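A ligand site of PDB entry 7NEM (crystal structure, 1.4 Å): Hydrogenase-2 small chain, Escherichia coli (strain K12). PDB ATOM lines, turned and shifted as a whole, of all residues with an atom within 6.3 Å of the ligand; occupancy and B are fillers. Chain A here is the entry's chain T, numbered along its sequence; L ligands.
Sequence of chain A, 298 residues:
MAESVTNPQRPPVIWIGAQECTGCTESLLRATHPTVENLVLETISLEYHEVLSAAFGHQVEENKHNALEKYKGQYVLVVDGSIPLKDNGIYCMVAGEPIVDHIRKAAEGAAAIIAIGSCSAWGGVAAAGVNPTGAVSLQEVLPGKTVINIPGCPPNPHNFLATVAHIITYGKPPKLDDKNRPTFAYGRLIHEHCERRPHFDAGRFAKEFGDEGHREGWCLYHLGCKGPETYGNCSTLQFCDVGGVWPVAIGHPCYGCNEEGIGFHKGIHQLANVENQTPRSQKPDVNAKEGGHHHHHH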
ATOM      1  N   ILE A 190      31.691 -26.739  24.320  1.00  0.00           N
ATOM      2  CA  ILE A 190      30.986 -25.637  25.013  1.00  0.00           C
ATOM      3  C   ILE A 190      30.352 -26.177  26.281  1.00  0.00           C
ATOM      4  O   ILE A 190      30.445 -25.541  27.316  1.00  0.00           O
ATOM      5  CB  ILE A 190      29.976 -24.979  24.046  1.00  0.00           C
ATOM      6  CG1 ILE A 190      30.752 -24.218  22.968  1.00  0.00           C
ATOM      7  CG2 ILE A 190      28.974 -24.147  24.808  1.00  0.00           C
ATOM      8  CD1 ILE A 190      29.872 -23.721  21.814  1.00  0.00           C
ATOM      9  N   HIS A 191      29.719 -27.357  26.239  1.00  0.00           N
ATOM     10  CA  HIS A 191      29.021 -27.938  27.397  1.00  0.00           C
ATOM     11  C   HIS A 191      29.996 -28.308  28.525  1.00  0.00           C
ATOM     12  O   HIS A 191      29.544 -28.461  29.665  1.00  0.00           O
ATOM     13  CB  HIS A 191      28.268 -29.178  26.921  1.00  0.00           C
ATOM     14  CG  HIS A 191      27.488 -29.919  27.946  1.00  0.00           C
ATOM     15  ND1 HIS A 191      26.261 -29.510  28.437  1.00  0.00           N
ATOM     16  CD2 HIS A 191      27.755 -31.146  28.479  1.00  0.00           C
ATOM     17  CE1 HIS A 191      25.838 -30.467  29.274  1.00  0.00           C
ATOM     18  NE2 HIS A 191      26.735 -31.450  29.306  1.00  0.00           N
ATOM     19  N   GLU A 192      31.277 -28.456  28.201  1.00  0.00           N
ATOM     20  CA  GLU A 192      32.313 -28.787  29.203  1.00  0.00           C
ATOM     21  C   GLU A 192      32.933 -27.514  29.763  1.00  0.00           C
ATOM     22  O   GLU A 192      33.901 -27.579  30.562  1.00  0.00           O
ATOM     23  CB  GLU A 192      33.407 -29.715  28.678  1.00  0.00           C
ATOM     24  CG  GLU A 192      32.849 -31.123  28.426  1.00  0.00           C
ATOM     25  CD  GLU A 192      32.177 -31.754  29.631  1.00  0.00           C
ATOM     26  OE1 GLU A 192      32.860 -31.857  30.658  1.00  0.00           O
ATOM     27  OE2 GLU A 192      30.998 -32.165  29.559  1.00  0.00           O
ATOM     28  N   CYS A 194      30.325 -24.572  30.296  1.00  0.00           N
ATOM     29  CA  CYS A 194      29.093 -23.762  30.214  1.00  0.00           C
ATOM     30  C   CYS A 194      28.569 -23.451  31.611  1.00  0.00           C
ATOM     31  O   CYS A 194      28.397 -24.373  32.434  1.00  0.00           O
ATOM     32  CB  CYS A 194      28.036 -24.517  29.404  1.00  0.00           C
ATOM     33  SG  CYS A 194      26.530 -23.553  29.319  1.00  0.00           S
ATOM     34  N   GLU A 195      28.298 -22.184  31.886  1.00  0.00           N
ATOM     35  CA  GLU A 195      27.840 -21.742  33.207  1.00  0.00           C
ATOM     36  C   GLU A 195      26.442 -22.264  33.543  1.00  0.00           C
ATOM     37  O   GLU A 195      26.054 -22.123  34.686  1.00  0.00           O
ATOM     38  CB  GLU A 195      27.890 -20.216  33.285  1.00  0.00           C
ATOM     39  CG  GLU A 195      26.922 -19.450  32.373  1.00  0.00           C
ATOM     40  CD  GLU A 195      27.285 -19.188  30.932  1.00  0.00           C
ATOM     41  OE1 GLU A 195      28.226 -19.816  30.431  1.00  0.00           O
ATOM     42  OE2 GLU A 195      26.621 -18.315  30.344  1.00  0.00           O
ATOM     43  N   ARG A 196      25.702 -22.849  32.585  1.00  0.00           N
ATOM     44  CA  ARG A 196      24.388 -23.451  32.928  1.00  0.00           C
ATOM     45  C   ARG A 196      24.516 -24.955  33.203  1.00  0.00           C
ATOM     46  O   ARG A 196      23.498 -25.577  33.463  1.00  0.00           O
ATOM     47  CB  ARG A 196      23.374 -23.190  31.814  1.00  0.00           C
ATOM     48  CG  ARG A 196      23.270 -21.707  31.529  1.00  0.00           C
ATOM     49  CD  ARG A 196      22.037 -21.322  30.746  1.00  0.00           C
ATOM     50  NE  ARG A 196      21.982 -19.856  30.634  1.00  0.00           N
ATOM     51  CZ  ARG A 196      20.881 -19.173  30.316  1.00  0.00           C
ATOM     52  NH1 ARG A 196      19.769 -19.790  29.961  1.00  0.00           N
ATOM     53  NH2 ARG A 196      20.937 -17.853  30.343  1.00  0.00           N
ATOM     54  N   ARG A 197      25.707 -25.482  33.202  1.00  0.00           N
ATOM     55  CA  ARG A 197      25.898 -26.922  33.543  1.00  0.00           C
ATOM     56  C   ARG A 197      25.286 -27.250  34.885  1.00  0.00           C
ATOM     57  O   ARG A 197      24.723 -28.352  35.036  1.00  0.00           O
ATOM     58  CB  ARG A 197      27.375 -27.279  33.449  1.00  0.00           C
ATOM     59  CG  ARG A 197      27.626 -28.727  33.843  1.00  0.00           C
ATOM     60  CD  ARG A 197      26.995 -29.725  32.867  1.00  0.00           C
ATOM     61  NE  ARG A 197      27.482 -31.064  33.164  1.00  0.00           N
ATOM     62  CZ  ARG A 197      28.549 -31.597  32.629  1.00  0.00           C
ATOM     63  NH1 ARG A 197      29.210 -31.033  31.635  1.00  0.00           N
ATOM     64  NH2 ARG A 197      28.988 -32.753  33.123  1.00  0.00           N
ATOM     65  N   PRO A 198      25.365 -26.434  35.962  1.00  0.00           N
ATOM     66  CA  PRO A 198      24.651 -26.792  37.201  1.00  0.00           C
ATOM     67  C   PRO A 198      23.176 -27.110  36.990  1.00  0.00           C
ATOM     68  O   PRO A 198      22.634 -28.002  37.656  1.00  0.00           O
ATOM     69  CB  PRO A 198      24.820 -25.575  38.093  1.00  0.00           C
ATOM     70  CG  PRO A 198      26.126 -24.920  37.573  1.00  0.00           C
ATOM     71  CD  PRO A 198      26.063 -25.143  36.073  1.00  0.00           C
ATOM     72  N   PHE A 200      21.718 -28.116  34.109  1.00  0.00           N
ATOM     73  CA  PHE A 200      21.708 -29.420  33.407  1.00  0.00           C
ATOM     74  C   PHE A 200      21.782 -30.525  34.467  1.00  0.00           C
ATOM     75  O   PHE A 200      20.958 -31.501  34.443  1.00  0.00           O
ATOM     76  CB  PHE A 200      22.873 -29.472  32.436  1.00  0.00           C
ATOM     77  CG  PHE A 200      22.969 -30.764  31.662  1.00  0.00           C
ATOM     78  CD1 PHE A 200      23.716 -31.808  32.162  1.00  0.00           C
ATOM     79  CD2 PHE A 200      22.384 -30.881  30.427  1.00  0.00           C
ATOM     80  CE1 PHE A 200      23.865 -32.990  31.449  1.00  0.00           C
ATOM     81  CE2 PHE A 200      22.523 -32.055  29.703  1.00  0.00           C
ATOM     82  CZ  PHE A 200      23.281 -33.094  30.196  1.00  0.00           C
ATOM     83  N   PHE A 205      15.590 -27.265  33.519  1.00  0.00           N
ATOM     84  CA  PHE A 205      15.578 -27.042  32.053  1.00  0.00           C
ATOM     85  C   PHE A 205      14.459 -26.068  31.653  1.00  0.00           C
ATOM     86  O   PHE A 205      13.297 -26.171  32.090  1.00  0.00           O
ATOM     87  CB  PHE A 205      15.267 -28.356  31.347  1.00  0.00           C
ATOM     88  CG  PHE A 205      16.332 -29.385  31.493  1.00  0.00           C
ATOM     89  CD1 PHE A 205      17.591 -29.192  30.978  1.00  0.00           C
ATOM     90  CD2 PHE A 205      16.069 -30.586  32.146  1.00  0.00           C
ATOM     91  CE1 PHE A 205      18.587 -30.140  31.145  1.00  0.00           C
ATOM     92  CE2 PHE A 205      17.046 -31.560  32.251  1.00  0.00           C
ATOM     93  CZ  PHE A 205      18.297 -31.333  31.757  1.00  0.00           C
ATOM     94  N   TRP A 218      17.826 -21.109  33.201  1.00  0.00           N
ATOM     95  CA  TRP A 218      18.126 -22.548  33.283  1.00  0.00           C
ATOM     96  C   TRP A 218      18.695 -23.088  31.968  1.00  0.00           C
ATOM     97  O   TRP A 218      18.854 -22.386  30.960  1.00  0.00           O
ATOM     98  CB  TRP A 218      16.863 -23.283  33.700  1.00  0.00           C
ATOM     99  CG  TRP A 218      16.411 -23.053  35.097  1.00  0.00           C
ATOM    100  CD1 TRP A 218      16.981 -22.289  36.055  1.00  0.00           C
ATOM    101  CD2 TRP A 218      15.274 -23.697  35.708  1.00  0.00           C
ATOM    102  NE1 TRP A 218      16.272 -22.405  37.236  1.00  0.00           N
ATOM    103  CE2 TRP A 218      15.212 -23.240  37.035  1.00  0.00           C
ATOM    104  CE3 TRP A 218      14.294 -24.588  35.234  1.00  0.00           C
ATOM    105  CZ2 TRP A 218      14.230 -23.677  37.928  1.00  0.00           C
ATOM    106  CZ3 TRP A 218      13.332 -25.022  36.120  1.00  0.00           C
ATOM    107  CH2 TRP A 218      13.303 -24.555  37.433  1.00  0.00           C
ATOM    108  N   CYS A 219      19.159 -24.326  31.994  1.00  0.00           N
ATOM    109  CA  CYS A 219      19.855 -24.962  30.883  1.00  0.00           C
ATOM    110  C   CYS A 219      18.912 -25.102  29.689  1.00  0.00           C
ATOM    111  O   CYS A 219      17.685 -25.313  29.898  1.00  0.00           O
ATOM    112  CB  CYS A 219      20.420 -26.311  31.330  1.00  0.00           C
ATOM    113  SG  CYS A 219      20.935 -27.426  29.992  1.00  0.00           S
ATOM    114  N   LEU A 220      19.451 -24.931  28.481  1.00  0.00           N
ATOM    115  CA  LEU A 220      18.685 -24.903  27.241  1.00  0.00           C
ATOM    116  C   LEU A 220      18.785 -26.238  26.495  1.00  0.00           C
ATOM    117  O   LEU A 220      18.400 -26.294  25.329  1.00  0.00           O
ATOM    118  CB  LEU A 220      19.136 -23.725  26.382  1.00  0.00           C
ATOM    119  CG  LEU A 220      19.157 -22.393  27.102  1.00  0.00           C
ATOM    120  CD1 LEU A 220      19.558 -21.296  26.102  1.00  0.00           C
ATOM    121  CD2 LEU A 220      17.821 -22.072  27.765  1.00  0.00           C
ATOM    122  N   TYR A 221      19.257 -27.303  27.144  1.00  0.00           N
ATOM    123  CA  TYR A 221      19.413 -28.637  26.471  1.00  0.00           C
ATOM    124  C   TYR A 221      18.101 -29.050  25.754  1.00  0.00           C
ATOM    125  O   TYR A 221      18.145 -29.486  24.581  1.00  0.00           O
ATOM    126  CB  TYR A 221      19.800 -29.697  27.495  1.00  0.00           C
ATOM    127  CG  TYR A 221      19.889 -31.034  26.809  1.00  0.00           C
ATOM    128  CD1 TYR A 221      21.000 -31.344  26.054  1.00  0.00           C
ATOM    129  CD2 TYR A 221      18.849 -31.958  26.853  1.00  0.00           C
ATOM    130  CE1 TYR A 221      21.072 -32.556  25.367  1.00  0.00           C
ATOM    131  CE2 TYR A 221      18.914 -33.158  26.163  1.00  0.00           C
ATOM    132  CZ  TYR A 221      20.034 -33.448  25.430  1.00  0.00           C
ATOM    133  OH  TYR A 221      20.089 -34.606  24.681  1.00  0.00           O
ATOM    134  N   HIS A 222      16.965 -28.941  26.455  1.00  0.00           N
ATOM    135  CA  HIS A 222      15.671 -29.437  25.902  1.00  0.00           C
ATOM    136  C   HIS A 222      15.064 -28.458  24.901  1.00  0.00           C
ATOM    137  O   HIS A 222      14.045 -28.836  24.282  1.00  0.00           O
ATOM    138  CB  HIS A 222      14.680 -29.847  26.989  1.00  0.00           C
ATOM    139  CG  HIS A 222      15.058 -31.163  27.570  1.00  0.00           C
ATOM    140  ND1 HIS A 222      14.846 -32.310  26.854  1.00  0.00           N
ATOM    141  CD2 HIS A 222      15.687 -31.500  28.723  1.00  0.00           C
ATOM    142  CE1 HIS A 222      15.322 -33.321  27.547  1.00  0.00           C
ATOM    143  NE2 HIS A 222      15.823 -32.866  28.723  1.00  0.00           N
ATOM    144  N   CYS A 225      19.895 -27.265  22.578  1.00  0.00           N
ATOM    145  CA  CYS A 225      21.292 -26.769  22.727  1.00  0.00           C
ATOM    146  C   CYS A 225      22.301 -27.798  22.192  1.00  0.00           C
ATOM    147  O   CYS A 225      22.320 -28.948  22.691  1.00  0.00           O
ATOM    148  CB  CYS A 225      21.582 -26.416  24.169  1.00  0.00           C
ATOM    149  SG  CYS A 225      23.200 -25.598  24.329  1.00  0.00           S
ATOM    150  N   LYS A 226      23.171 -27.384  21.298  1.00  0.00           N
ATOM    151  CA  LYS A 226      24.190 -28.266  20.698  1.00  0.00           C
ATOM    152  C   LYS A 226      25.513 -28.117  21.432  1.00  0.00           C
ATOM    153  O   LYS A 226      26.533 -28.690  20.984  1.00  0.00           O
ATOM    154  CB  LYS A 226      24.373 -28.011  19.215  1.00  0.00           C
ATOM    155  CG  LYS A 226      23.078 -28.158  18.403  1.00  0.00           C
ATOM    156  CD  LYS A 226      22.320 -29.437  18.689  1.00  0.00           C
ATOM    157  CE  LYS A 226      21.214 -29.687  17.693  1.00  0.00           C
ATOM    158  NZ  LYS A 226      20.213 -28.601  17.740  1.00  0.00           N
ATOM    159  N   GLY A 227      25.544 -27.385  22.548  1.00  0.00           N
ATOM    160  CA  GLY A 227      26.797 -27.291  23.327  1.00  0.00           C
ATOM    161  C   GLY A 227      27.463 -28.630  23.626  1.00  0.00           C
ATOM    162  O   GLY A 227      28.697 -28.709  23.615  1.00  0.00           O
ATOM    163  N   PRO A 228      26.693 -29.701  23.918  1.00  0.00           N
ATOM    164  CA  PRO A 228      27.308 -31.006  24.173  1.00  0.00           C
ATOM    165  C   PRO A 228      28.088 -31.619  23.027  1.00  0.00           C
ATOM    166  O   PRO A 228      28.874 -32.545  23.273  1.00  0.00           O
ATOM    167  CB  PRO A 228      26.146 -31.892  24.577  1.00  0.00           C
ATOM    168  CG  PRO A 228      25.099 -30.930  25.073  1.00  0.00           C
ATOM    169  CD  PRO A 228      25.269 -29.698  24.211  1.00  0.00           C
ATOM    170  N   TRP A 246      26.568 -14.179  24.692  1.00  0.00           N
ATOM    171  CA  TRP A 246      26.660 -15.327  23.792  1.00  0.00           C
ATOM    172  C   TRP A 246      25.276 -15.892  23.645  1.00  0.00           C
ATOM    173  O   TRP A 246      24.347 -15.490  24.385  1.00  0.00           O
ATOM    174  CB  TRP A 246      27.695 -16.352  24.216  1.00  0.00           C
ATOM    175  CG  TRP A 246      27.389 -17.214  25.416  1.00  0.00           C
ATOM    176  CD1 TRP A 246      27.359 -16.859  26.731  1.00  0.00           C
ATOM    177  CD2 TRP A 246      27.252 -18.650  25.418  1.00  0.00           C
ATOM    178  NE1 TRP A 246      27.200 -17.948  27.542  1.00  0.00           N
ATOM    179  CE2 TRP A 246      27.106 -19.049  26.758  1.00  0.00           C
ATOM    180  CE3 TRP A 246      27.189 -19.598  24.403  1.00  0.00           C
ATOM    181  CZ2 TRP A 246      26.993 -20.405  27.102  1.00  0.00           C
ATOM    182  CZ3 TRP A 246      27.082 -20.928  24.733  1.00  0.00           C
ATOM    183  CH2 TRP A 246      26.972 -21.304  26.064  1.00  0.00           C
ATOM    184  N   VAL A 248      23.515 -18.596  24.309  1.00  0.00           N
ATOM    185  CA  VAL A 248      22.877 -19.236  25.485  1.00  0.00           C
ATOM    186  C   VAL A 248      22.617 -18.162  26.559  1.00  0.00           C
ATOM    187  O   VAL A 248      21.533 -18.170  27.157  1.00  0.00           O
ATOM    188  CB  VAL A 248      23.724 -20.412  25.986  1.00  0.00           C
ATOM    189  CG1 VAL A 248      23.359 -20.846  27.397  1.00  0.00           C
ATOM    190  CG2 VAL A 248      23.604 -21.586  25.015  1.00  0.00           C
ATOM    191  N   PRO A 253      19.385 -21.644  22.535  1.00  0.00           N
ATOM    192  CA  PRO A 253      20.352 -22.729  22.476  1.00  0.00           C
ATOM    193  C   PRO A 253      21.460 -22.448  21.473  1.00  0.00           C
ATOM    194  O   PRO A 253      21.273 -21.790  20.444  1.00  0.00           O
ATOM    195  CB  PRO A 253      19.528 -23.945  21.977  1.00  0.00           C
ATOM    196  CG  PRO A 253      18.283 -23.322  21.380  1.00  0.00           C
ATOM    197  CD  PRO A 253      18.014 -22.074  22.204  1.00  0.00           C
ATOM    198  N   CYS A 254      22.637 -22.999  21.768  1.00  0.00           N
ATOM    199  CA  CYS A 254      23.682 -23.211  20.744  1.00  0.00           C
ATOM    200  C   CYS A 254      23.074 -24.059  19.597  1.00  0.00           C
ATOM    201  O   CYS A 254      22.365 -25.050  19.870  1.00  0.00           O
ATOM    202  CB  CYS A 254      24.930 -23.867  21.343  1.00  0.00           C
ATOM    203  SG  CYS A 254      26.222 -24.315  20.138  1.00  0.00           S
HETATM  204 FE1  LIG L   1      22.860 -26.679  29.026  1.00  0.00          FE
HETATM  205 FE2  LIG L   1      23.747 -26.071  26.478  1.00  0.00          FE
HETATM  206 FE3  LIG L   1      25.169 -27.804  28.072  1.00  0.00          FE
HETATM  207 FE4  LIG L   1      25.090 -25.165  28.682  1.00  0.00          FE
HETATM  208  S1  LIG L   1      26.014 -26.152  26.791  1.00  0.00           S
HETATM  209  S2  LIG L   1      24.819 -26.847  30.136  1.00  0.00           S
HETATM  210  S3  LIG L   1      22.937 -24.624  28.107  1.00  0.00           S
HETATM  211  S4  LIG L   1      23.077 -28.105  27.199  1.00  0.00           S
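The backbone carbonyl oxygen of Arg 196 lies close to a sulfur (S2) of the ligand, 3.8 Å away.
Phe 200 touches the ligand.
Tyr 221 touches the ligand (CB to S4, 3.7 Å).
Gly 227 touches the ligand.
Val 248 touches the ligand (CG1 to S3, 3.9 Å).
Hydrophobic or aromatic side chains that line the ligand: His 191, Phe 200, Tyr 221 and Val 248.
The nearest printed residue that does not touch the ligand is Pro 228 (4.03 Å).
A ring nitrogen (ND1) of His 191 is bound to an iron atom (FE3) of the ligand (2.1 Å).
The side-chain sulfur (SG) of Cys 194 is bound to an iron atom (FE4) of the ligand, at 2.3 Å.
FE2 of the ligand is bound by SG of Cys 225 (2.3 Å).
SG of Cys 219 binds FE1 of the ligand, 2.3 Å away.
A sulfur (S2) of the ligand sits close to the backbone NH of Arg 197, 3.5 Å away.
N of Leu 220 lies close to S3 of the ligand (3.5 Å).
The guanidinium group (NH1) of Arg 197 sits at hydrogen-bond distance from the backbone carbonyl oxygen (O) of His 191 (3.3 Å).
The backbone carbonyl oxygen of Gly 227 is in hydrogen-bond range of the backbone NH of His 191.
The side-chain sulfur (SG) of Cys 194 sits close to the backbone NH (N) of Arg 196 (3.4 Å).
The side-chain sulfur of Cys 225 sits close to the backbone NH of Gly 227 (3.4 Å).
The side-chain sulfur (SG) of Cys 225 lies close to the backbone NH (N) of Cys 254 (3.7 Å).
The guanidinium group (NH1) of Arg 197 is in salt-bridge range of the side-chain carboxylate (OE2) of Glu 192 (3.0 Å).
The guanidinium group (NH2) of Arg 196 sits at hydrogen-bond distance from the backbone carbonyl oxygen (O) of Val 248 (3.3 Å).
The backbone carbonyl oxygen (O) of Trp 218 lies within hydrogen-bond range of the guanidinium group (NH1) of Arg 196, at 2.9 Å.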
